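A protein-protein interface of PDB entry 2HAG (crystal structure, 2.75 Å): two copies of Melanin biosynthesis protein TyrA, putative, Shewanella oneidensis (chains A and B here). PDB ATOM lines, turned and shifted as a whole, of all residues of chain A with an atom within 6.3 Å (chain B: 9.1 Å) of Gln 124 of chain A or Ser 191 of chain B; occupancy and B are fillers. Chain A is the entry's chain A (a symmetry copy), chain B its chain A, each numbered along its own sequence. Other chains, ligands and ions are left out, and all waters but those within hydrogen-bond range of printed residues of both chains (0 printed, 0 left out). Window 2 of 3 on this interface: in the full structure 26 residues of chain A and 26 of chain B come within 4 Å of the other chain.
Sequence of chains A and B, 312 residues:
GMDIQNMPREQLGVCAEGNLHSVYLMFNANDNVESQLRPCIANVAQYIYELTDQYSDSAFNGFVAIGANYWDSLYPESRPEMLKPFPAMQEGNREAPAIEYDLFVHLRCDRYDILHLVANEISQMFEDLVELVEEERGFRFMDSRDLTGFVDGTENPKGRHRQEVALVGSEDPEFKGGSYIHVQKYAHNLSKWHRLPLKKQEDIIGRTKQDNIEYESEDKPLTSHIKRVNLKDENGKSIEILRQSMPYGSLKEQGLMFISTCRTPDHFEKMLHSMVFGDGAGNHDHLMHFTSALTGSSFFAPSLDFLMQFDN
Printed residues of chain A within 4 Å of Ser 191 of chain B: Gln 124 (3.4 Å). Of chain B, only Leu 251 (3.6 Å) comes within 4 Å of Ser 123 of chain A. Of the printed residues of chain B, Asn 120 of chain A touches Leu 251 and Gln 254. Of the printed residues of chain B, Ala 119 of chain A touches Leu 251 (3.7 Å). Of the printed residues of chain A, Gln 254 of chain B touches Asn 120. Of the printed residues of chain A, Leu 251 of chain B touches Ala 119, Asn 120 and Ser 123. The nearest residue of chain B that does not touch Gln 124 of chain A is Leu 190 of chain B (5.4 Å).
The side-chain amide nitrogen of Asn 120 of chain A lies within hydrogen-bond range of the side-chain amide oxygen of Gln 254 of chain B (3.0 Å).
The backbone NH (N) of His 188 of chain B sits at hydrogen-bond distance from the backbone carbonyl oxygen (O) of Gln 254 of chain B, at 2.8 Å. OD1 of Asn 189 of chain B sits at hydrogen-bond distance from OG of Ser 191 of chain B.
Leu 251 of chain B touches Ala 119 of chain A. OD1 of Asn 120 of chain A touches CD2 of Leu 251 of chain B (3.3 Å). Leu 251 of chain B touches Ser 123 of chain A. NE2 of Gln 124 of chain A touches CB of Ser 191 of chain B, 3.4 Å away.
No position is printed for both chains. Of the 5 pairs that touch across the chains among the printed residues, none has its exchanged pair printed and touching as well.
Along chain B the printed residues that touch a printed residue of chain A span positions 191 to 254. Of the 9 printed residues of chain A, 4 touch a printed residue of chain B. Printed residues of chain A that touch a printed residue of chain B: Ala 119, Asn 120, Ser 123 and Gln 124. Among the printed residues, no Asp or Glu carboxylate lies within 4 Å of a Lys or Arg side-chain nitrogen of the other chain.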
ATOM      1  N   ALA A 119     -24.589  16.844 -12.307  1.00  0.00           N
ATOM      2  CA  ALA A 119     -25.321  18.103 -12.423  1.00  0.00           C
ATOM      3  C   ALA A 119     -24.704  19.017 -13.510  1.00  0.00           C
ATOM      4  O   ALA A 119     -25.416  19.504 -14.383  1.00  0.00           O
ATOM      5  CB  ALA A 119     -25.362  18.804 -11.077  1.00  0.00           C
ATOM      6  N   ASN A 120     -23.388  19.232 -13.460  1.00  0.00           N
ATOM      7  CA  ASN A 120     -22.691  19.982 -14.507  1.00  0.00           C
ATOM      8  C   ASN A 120     -22.952  19.408 -15.895  1.00  0.00           C
ATOM      9  O   ASN A 120     -23.162  20.137 -16.863  1.00  0.00           O
ATOM     10  CB  ASN A 120     -21.180  19.981 -14.267  1.00  0.00           C
ATOM     11  CG  ASN A 120     -20.758  20.963 -13.203  1.00  0.00           C
ATOM     12  OD1 ASN A 120     -21.473  21.904 -12.901  1.00  0.00           O
ATOM     13  ND2 ASN A 120     -19.589  20.747 -12.632  1.00  0.00           N
ATOM     14  N   GLU A 121     -22.925  18.089 -15.988  1.00  0.00           N
ATOM     15  CA  GLU A 121     -23.021  17.430 -17.266  1.00  0.00           C
ATOM     16  C   GLU A 121     -24.419  17.599 -17.822  1.00  0.00           C
ATOM     17  O   GLU A 121     -24.594  17.790 -19.024  1.00  0.00           O
ATOM     18  CB  GLU A 121     -22.669  15.951 -17.110  1.00  0.00           C
ATOM     19  CG  GLU A 121     -22.614  15.168 -18.420  1.00  0.00           C
ATOM     20  CD  GLU A 121     -21.517  15.639 -19.372  1.00  0.00           C
ATOM     21  OE1 GLU A 121     -20.366  15.851 -18.913  1.00  0.00           O
ATOM     22  OE2 GLU A 121     -21.818  15.776 -20.584  1.00  0.00           O
ATOM     23  N   ILE A 122     -25.415  17.547 -16.947  1.00  0.00           N
ATOM     24  CA  ILE A 122     -26.796  17.664 -17.391  1.00  0.00           C
ATOM     25  C   ILE A 122     -27.078  19.090 -17.816  1.00  0.00           C
ATOM     26  O   ILE A 122     -27.728  19.332 -18.837  1.00  0.00           O
ATOM     27  CB  ILE A 122     -27.798  17.252 -16.304  1.00  0.00           C
ATOM     28  CG1 ILE A 122     -27.746  15.734 -16.088  1.00  0.00           C
ATOM     29  CG2 ILE A 122     -29.200  17.667 -16.709  1.00  0.00           C
ATOM     30  CD1 ILE A 122     -28.471  15.247 -14.850  1.00  0.00           C
ATOM     31  N   SER A 123     -26.591  20.037 -17.028  1.00  0.00           N
ATOM     32  CA  SER A 123     -26.665  21.440 -17.408  1.00  0.00           C
ATOM     33  C   SER A 123     -26.050  21.667 -18.790  1.00  0.00           C
ATOM     34  O   SER A 123     -26.663  22.285 -19.655  1.00  0.00           O
ATOM     35  CB  SER A 123     -25.943  22.313 -16.383  1.00  0.00           C
ATOM     36  OG  SER A 123     -25.594  23.556 -16.964  1.00  0.00           O
ATOM     37  N   GLN A 124     -24.837  21.162 -18.991  1.00  0.00           N
ATOM     38  CA  GLN A 124     -24.136  21.357 -20.251  1.00  0.00           C
ATOM     39  C   GLN A 124     -24.925  20.678 -21.360  1.00  0.00           C
ATOM     40  O   GLN A 124     -24.825  21.062 -22.523  1.00  0.00           O
ATOM     41  CB  GLN A 124     -22.704  20.812 -20.178  1.00  0.00           C
ATOM     42  CG  GLN A 124     -21.735  21.514 -21.117  1.00  0.00           C
ATOM     43  CD  GLN A 124     -20.317  21.669 -20.542  1.00  0.00           C
ATOM     44  OE1 GLN A 124     -19.841  20.831 -19.763  1.00  0.00           O
ATOM     45  NE2 GLN A 124     -19.635  22.747 -20.939  1.00  0.00           N
ATOM     46  N   MET A 125     -25.724  19.679 -20.996  1.00  0.00           N
ATOM     47  CA  MET A 125     -26.532  18.977 -21.981  1.00  0.00           C
ATOM     48  C   MET A 125     -27.649  19.867 -22.479  1.00  0.00           C
ATOM     49  O   MET A 125     -27.837  19.991 -23.673  1.00  0.00           O
ATOM     50  CB  MET A 125     -27.084  17.663 -21.427  1.00  0.00           C
ATOM     51  CG  MET A 125     -26.092  16.506 -21.544  1.00  0.00           C
ATOM     52  SD  MET A 125     -26.579  14.824 -20.614  1.00  0.00           S
ATOM     53  CE  MET A 125     -27.702  13.978 -21.975  1.00  0.00           C
ATOM     54  N   PHE A 126     -28.375  20.517 -21.581  1.00  0.00           N
ATOM     55  CA  PHE A 126     -29.502  21.362 -22.001  1.00  0.00           C
ATOM     56  C   PHE A 126     -29.098  22.554 -22.875  1.00  0.00           C
ATOM     57  O   PHE A 126     -29.959  23.227 -23.447  1.00  0.00           O
ATOM     58  CB  PHE A 126     -30.284  21.869 -20.793  1.00  0.00           C
ATOM     59  CG  PHE A 126     -31.166  20.830 -20.161  1.00  0.00           C
ATOM     60  CD1 PHE A 126     -32.183  20.241 -20.879  1.00  0.00           C
ATOM     61  CD2 PHE A 126     -30.990  20.459 -18.850  1.00  0.00           C
ATOM     62  CE1 PHE A 126     -32.997  19.297 -20.301  1.00  0.00           C
ATOM     63  CE2 PHE A 126     -31.800  19.521 -18.275  1.00  0.00           C
ATOM     64  CZ  PHE A 126     -32.804  18.939 -18.998  1.00  0.00           C
ATOM     65  N   GLU A 127     -27.799  22.815 -22.979  1.00  0.00           N
ATOM     66  CA  GLU A 127     -27.300  23.866 -23.869  1.00  0.00           C
ATOM     67  C   GLU A 127     -27.945  25.217 -23.537  1.00  0.00           C
ATOM     68  O   GLU A 127     -27.900  25.660 -22.394  1.00  0.00           O
ATOM     69  CB  GLU A 127     -27.517  23.489 -25.352  1.00  0.00           C
ATOM     70  CG  GLU A 127     -26.862  22.156 -25.774  1.00  0.00           C
ATOM     71  CD  GLU A 127     -26.364  22.147 -27.219  1.00  0.00           C
ATOM     72  OE1 GLU A 127     -26.812  23.001 -28.022  1.00  0.00           O
ATOM     73  OE2 GLU A 127     -25.522  21.280 -27.549  1.00  0.00           O
ATOM     74  N   LEU B 147     -12.016  21.079  -9.673  1.00  0.00           N
ATOM     75  CA  LEU B 147     -13.073  20.903 -10.677  1.00  0.00           C
ATOM     76  C   LEU B 147     -12.507  20.995 -12.081  1.00  0.00           C
ATOM     77  O   LEU B 147     -13.151  20.633 -13.073  1.00  0.00           O
ATOM     78  CB  LEU B 147     -14.148  21.966 -10.486  1.00  0.00           C
ATOM     79  CG  LEU B 147     -14.892  21.854  -9.163  1.00  0.00           C
ATOM     80  CD1 LEU B 147     -15.854  23.025  -8.992  1.00  0.00           C
ATOM     81  CD2 LEU B 147     -15.628  20.529  -9.124  1.00  0.00           C
ATOM     82  N   THR B 148     -11.286  21.497 -12.136  1.00  0.00           N
ATOM     83  CA  THR B 148     -10.516  21.540 -13.346  1.00  0.00           C
ATOM     84  C   THR B 148     -10.066  20.135 -13.779  1.00  0.00           C
ATOM     85  O   THR B 148      -9.695  19.921 -14.929  1.00  0.00           O
ATOM     86  CB  THR B 148      -9.321  22.464 -13.139  1.00  0.00           C
ATOM     87  OG1 THR B 148      -8.832  22.875 -14.413  1.00  0.00           O
ATOM     88  CG2 THR B 148      -8.234  21.780 -12.357  1.00  0.00           C
ATOM     89  N   HIS B 188     -14.476  29.217 -11.346  1.00  0.00           N
ATOM     90  CA  HIS B 188     -13.982  28.631 -12.575  1.00  0.00           C
ATOM     91  C   HIS B 188     -14.968  28.824 -13.694  1.00  0.00           C
ATOM     92  O   HIS B 188     -16.173  28.681 -13.509  1.00  0.00           O
ATOM     93  CB  HIS B 188     -13.748  27.138 -12.412  1.00  0.00           C
ATOM     94  CG  HIS B 188     -12.610  26.796 -11.508  1.00  0.00           C
ATOM     95  ND1 HIS B 188     -12.290  27.544 -10.399  1.00  0.00           N
ATOM     96  CD2 HIS B 188     -11.738  25.763 -11.532  1.00  0.00           C
ATOM     97  CE1 HIS B 188     -11.261  26.992  -9.786  1.00  0.00           C
ATOM     98  NE2 HIS B 188     -10.910  25.907 -10.451  1.00  0.00           N
ATOM     99  N   ASN B 189     -14.439  29.153 -14.858  1.00  0.00           N
ATOM    100  CA  ASN B 189     -15.208  29.114 -16.069  1.00  0.00           C
ATOM    101  C   ASN B 189     -15.041  27.717 -16.675  1.00  0.00           C
ATOM    102  O   ASN B 189     -14.282  27.510 -17.616  1.00  0.00           O
ATOM    103  CB  ASN B 189     -14.713  30.205 -17.005  1.00  0.00           C
ATOM    104  CG  ASN B 189     -15.524  30.286 -18.273  1.00  0.00           C
ATOM    105  OD1 ASN B 189     -16.343  29.407 -18.561  1.00  0.00           O
ATOM    106  ND2 ASN B 189     -15.295  31.339 -19.047  1.00  0.00           N
ATOM    107  N   LEU B 190     -15.746  26.746 -16.114  1.00  0.00           N
ATOM    108  CA  LEU B 190     -15.491  25.347 -16.446  1.00  0.00           C
ATOM    109  C   LEU B 190     -15.781  24.974 -17.894  1.00  0.00           C
ATOM    110  O   LEU B 190     -15.049  24.181 -18.478  1.00  0.00           O
ATOM    111  CB  LEU B 190     -16.264  24.429 -15.509  1.00  0.00           C
ATOM    112  CG  LEU B 190     -15.671  24.268 -14.106  1.00  0.00           C
ATOM    113  CD1 LEU B 190     -16.534  23.365 -13.263  1.00  0.00           C
ATOM    114  CD2 LEU B 190     -14.269  23.706 -14.164  1.00  0.00           C
ATOM    115  N   SER B 191     -16.830  25.527 -18.491  1.00  0.00           N
ATOM    116  CA  SER B 191     -17.113  25.198 -19.887  1.00  0.00           C
ATOM    117  C   SER B 191     -15.979  25.668 -20.792  1.00  0.00           C
ATOM    118  O   SER B 191     -15.639  24.992 -21.755  1.00  0.00           O
ATOM    119  CB  SER B 191     -18.419  25.817 -20.344  1.00  0.00           C
ATOM    120  OG  SER B 191     -18.448  27.163 -19.949  1.00  0.00           O
ATOM    121  N   LYS B 192     -15.392  26.817 -20.478  1.00  0.00           N
ATOM    122  CA  LYS B 192     -14.249  27.323 -21.241  1.00  0.00           C
ATOM    123  C   LYS B 192     -13.057  26.417 -21.037  1.00  0.00           C
ATOM    124  O   LYS B 192     -12.294  26.143 -21.965  1.00  0.00           O
ATOM    125  CB  LYS B 192     -13.885  28.738 -20.795  1.00  0.00           C
ATOM    126  CG  LYS B 192     -12.767  29.367 -21.579  1.00  0.00           C
ATOM    127  CD  LYS B 192     -12.508  30.783 -21.108  1.00  0.00           C
ATOM    128  CE  LYS B 192     -11.327  31.384 -21.862  1.00  0.00           C
ATOM    129  NZ  LYS B 192     -11.124  32.813 -21.559  1.00  0.00           N
ATOM    130  N   TRP B 193     -12.903  25.949 -19.810  1.00  0.00           N
ATOM    131  CA  TRP B 193     -11.775  25.120 -19.475  1.00  0.00           C
ATOM    132  C   TRP B 193     -11.853  23.774 -20.171  1.00  0.00           C
ATOM    133  O   TRP B 193     -10.892  23.324 -20.801  1.00  0.00           O
ATOM    134  CB  TRP B 193     -11.697  24.902 -17.972  1.00  0.00           C
ATOM    135  CG  TRP B 193     -10.605  23.957 -17.613  1.00  0.00           C
ATOM    136  CD1 TRP B 193     -10.732  22.639 -17.307  1.00  0.00           C
ATOM    137  CD2 TRP B 193      -9.212  24.252 -17.548  1.00  0.00           C
ATOM    138  NE1 TRP B 193      -9.505  22.095 -17.047  1.00  0.00           N
ATOM    139  CE2 TRP B 193      -8.552  23.066 -17.189  1.00  0.00           C
ATOM    140  CE3 TRP B 193      -8.455  25.406 -17.761  1.00  0.00           C
ATOM    141  CZ2 TRP B 193      -7.176  23.001 -17.034  1.00  0.00           C
ATOM    142  CZ3 TRP B 193      -7.086  25.340 -17.604  1.00  0.00           C
ATOM    143  CH2 TRP B 193      -6.461  24.147 -17.244  1.00  0.00           C
ATOM    144  N   HIS B 194     -13.001  23.125 -20.064  1.00  0.00           N
ATOM    145  CA  HIS B 194     -13.100  21.752 -20.544  1.00  0.00           C
ATOM    146  C   HIS B 194     -13.221  21.660 -22.062  1.00  0.00           C
ATOM    147  O   HIS B 194     -13.322  20.563 -22.602  1.00  0.00           O
ATOM    148  CB  HIS B 194     -14.218  20.990 -19.814  1.00  0.00           C
ATOM    149  CG  HIS B 194     -13.863  20.640 -18.402  1.00  0.00           C
ATOM    150  ND1 HIS B 194     -12.823  19.788 -18.087  1.00  0.00           N
ATOM    151  CD2 HIS B 194     -14.384  21.050 -17.220  1.00  0.00           C
ATOM    152  CE1 HIS B 194     -12.729  19.680 -16.772  1.00  0.00           C
ATOM    153  NE2 HIS B 194     -13.665  20.436 -16.224  1.00  0.00           N
ATOM    154  N   ARG B 195     -13.171  22.807 -22.742  1.00  0.00           N
ATOM    155  CA  ARG B 195     -13.055  22.831 -24.201  1.00  0.00           C
ATOM    156  C   ARG B 195     -11.596  22.890 -24.633  1.00  0.00           C
ATOM    157  O   ARG B 195     -11.298  22.923 -25.812  1.00  0.00           O
ATOM    158  CB  ARG B 195     -13.816  24.012 -24.807  1.00  0.00           C
ATOM    159  CG  ARG B 195     -15.262  24.066 -24.391  1.00  0.00           C
ATOM    160  CD  ARG B 195     -16.134  24.795 -25.388  1.00  0.00           C
ATOM    161  NE  ARG B 195     -16.302  24.026 -26.612  1.00  0.00           N
ATOM    162  CZ  ARG B 195     -17.114  24.369 -27.606  1.00  0.00           C
ATOM    163  NH1 ARG B 195     -17.855  25.465 -27.524  1.00  0.00           N
ATOM    164  NH2 ARG B 195     -17.196  23.611 -28.686  1.00  0.00           N
ATOM    165  N   LEU B 196     -10.674  22.911 -23.691  1.00  0.00           N
ATOM    166  CA  LEU B 196      -9.280  22.819 -24.073  1.00  0.00           C
ATOM    167  C   LEU B 196      -8.937  21.357 -24.287  1.00  0.00           C
ATOM    168  O   LEU B 196      -9.369  20.510 -23.513  1.00  0.00           O
ATOM    169  CB  LEU B 196      -8.377  23.403 -22.985  1.00  0.00           C
ATOM    170  CG  LEU B 196      -8.600  24.868 -22.615  1.00  0.00           C
ATOM    171  CD1 LEU B 196      -7.498  25.320 -21.670  1.00  0.00           C
ATOM    172  CD2 LEU B 196      -8.643  25.743 -23.854  1.00  0.00           C
ATOM    173  N   GLN B 201      -4.567  21.944 -21.529  1.00  0.00           N
ATOM    174  CA  GLN B 201      -4.839  21.939 -20.096  1.00  0.00           C
ATOM    175  C   GLN B 201      -3.545  21.641 -19.343  1.00  0.00           C
ATOM    176  O   GLN B 201      -3.177  22.361 -18.418  1.00  0.00           O
ATOM    177  CB  GLN B 201      -5.920  20.904 -19.721  1.00  0.00           C
ATOM    178  CG  GLN B 201      -7.353  21.305 -20.091  1.00  0.00           C
ATOM    179  CD  GLN B 201      -8.432  20.338 -19.582  1.00  0.00           C
ATOM    180  OE1 GLN B 201      -8.207  19.541 -18.665  1.00  0.00           O
ATOM    181  NE2 GLN B 201      -9.621  20.424 -20.174  1.00  0.00           N
ATOM    182  N   LEU B 251     -24.048  24.950  -9.698  1.00  0.00           N
ATOM    183  CA  LEU B 251     -24.100  25.363 -11.088  1.00  0.00           C
ATOM    184  C   LEU B 251     -24.020  26.864 -11.203  1.00  0.00           C
ATOM    185  O   LEU B 251     -23.397  27.370 -12.117  1.00  0.00           O
ATOM    186  CB  LEU B 251     -25.379  24.885 -11.763  1.00  0.00           C
ATOM    187  CG  LEU B 251     -25.536  23.384 -12.011  1.00  0.00           C
ATOM    188  CD1 LEU B 251     -26.970  23.088 -12.384  1.00  0.00           C
ATOM    189  CD2 LEU B 251     -24.603  22.889 -13.102  1.00  0.00           C
ATOM    190  N   GLN B 254     -19.169  27.991  -9.308  1.00  0.00           N
ATOM    191  CA  GLN B 254     -18.340  26.959  -8.697  1.00  0.00           C
ATOM    192  C   GLN B 254     -16.861  27.195  -8.979  1.00  0.00           C
ATOM    193  O   GLN B 254     -16.493  27.880  -9.940  1.00  0.00           O
ATOM    194  CB  GLN B 254     -18.740  25.582  -9.234  1.00  0.00           C
ATOM    195  CG  GLN B 254     -18.534  25.434 -10.729  1.00  0.00           C
ATOM    196  CD  GLN B 254     -19.257  24.239 -11.291  1.00  0.00           C
ATOM    197  OE1 GLN B 254     -18.928  23.099 -10.972  1.00  0.00           O
ATOM    198  NE2 GLN B 254     -20.252  24.491 -12.133  1.00  0.00           N
ATOM    199  N   PHE B 290      -8.993  31.236 -16.945  1.00  0.00           N
ATOM    200  CA  PHE B 290     -10.053  30.261 -16.846  1.00  0.00           C
ATOM    201  C   PHE B 290     -10.791  30.298 -15.524  1.00  0.00           C
ATOM    202  O   PHE B 290     -11.758  29.564 -15.327  1.00  0.00           O
ATOM    203  CB  PHE B 290      -9.460  28.881 -17.132  1.00  0.00           C
ATOM    204  CG  PHE B 290      -8.846  28.788 -18.499  1.00  0.00           C
ATOM    205  CD1 PHE B 290      -9.632  28.521 -19.611  1.00  0.00           C
ATOM    206  CD2 PHE B 290      -7.506  29.029 -18.687  1.00  0.00           C
ATOM    207  CE1 PHE B 290      -9.078  28.469 -20.873  1.00  0.00           C
ATOM    208  CE2 PHE B 290      -6.953  28.979 -19.955  1.00  0.00           C
ATOM    209  CZ  PHE B 290      -7.737  28.699 -21.040  1.00  0.00           C
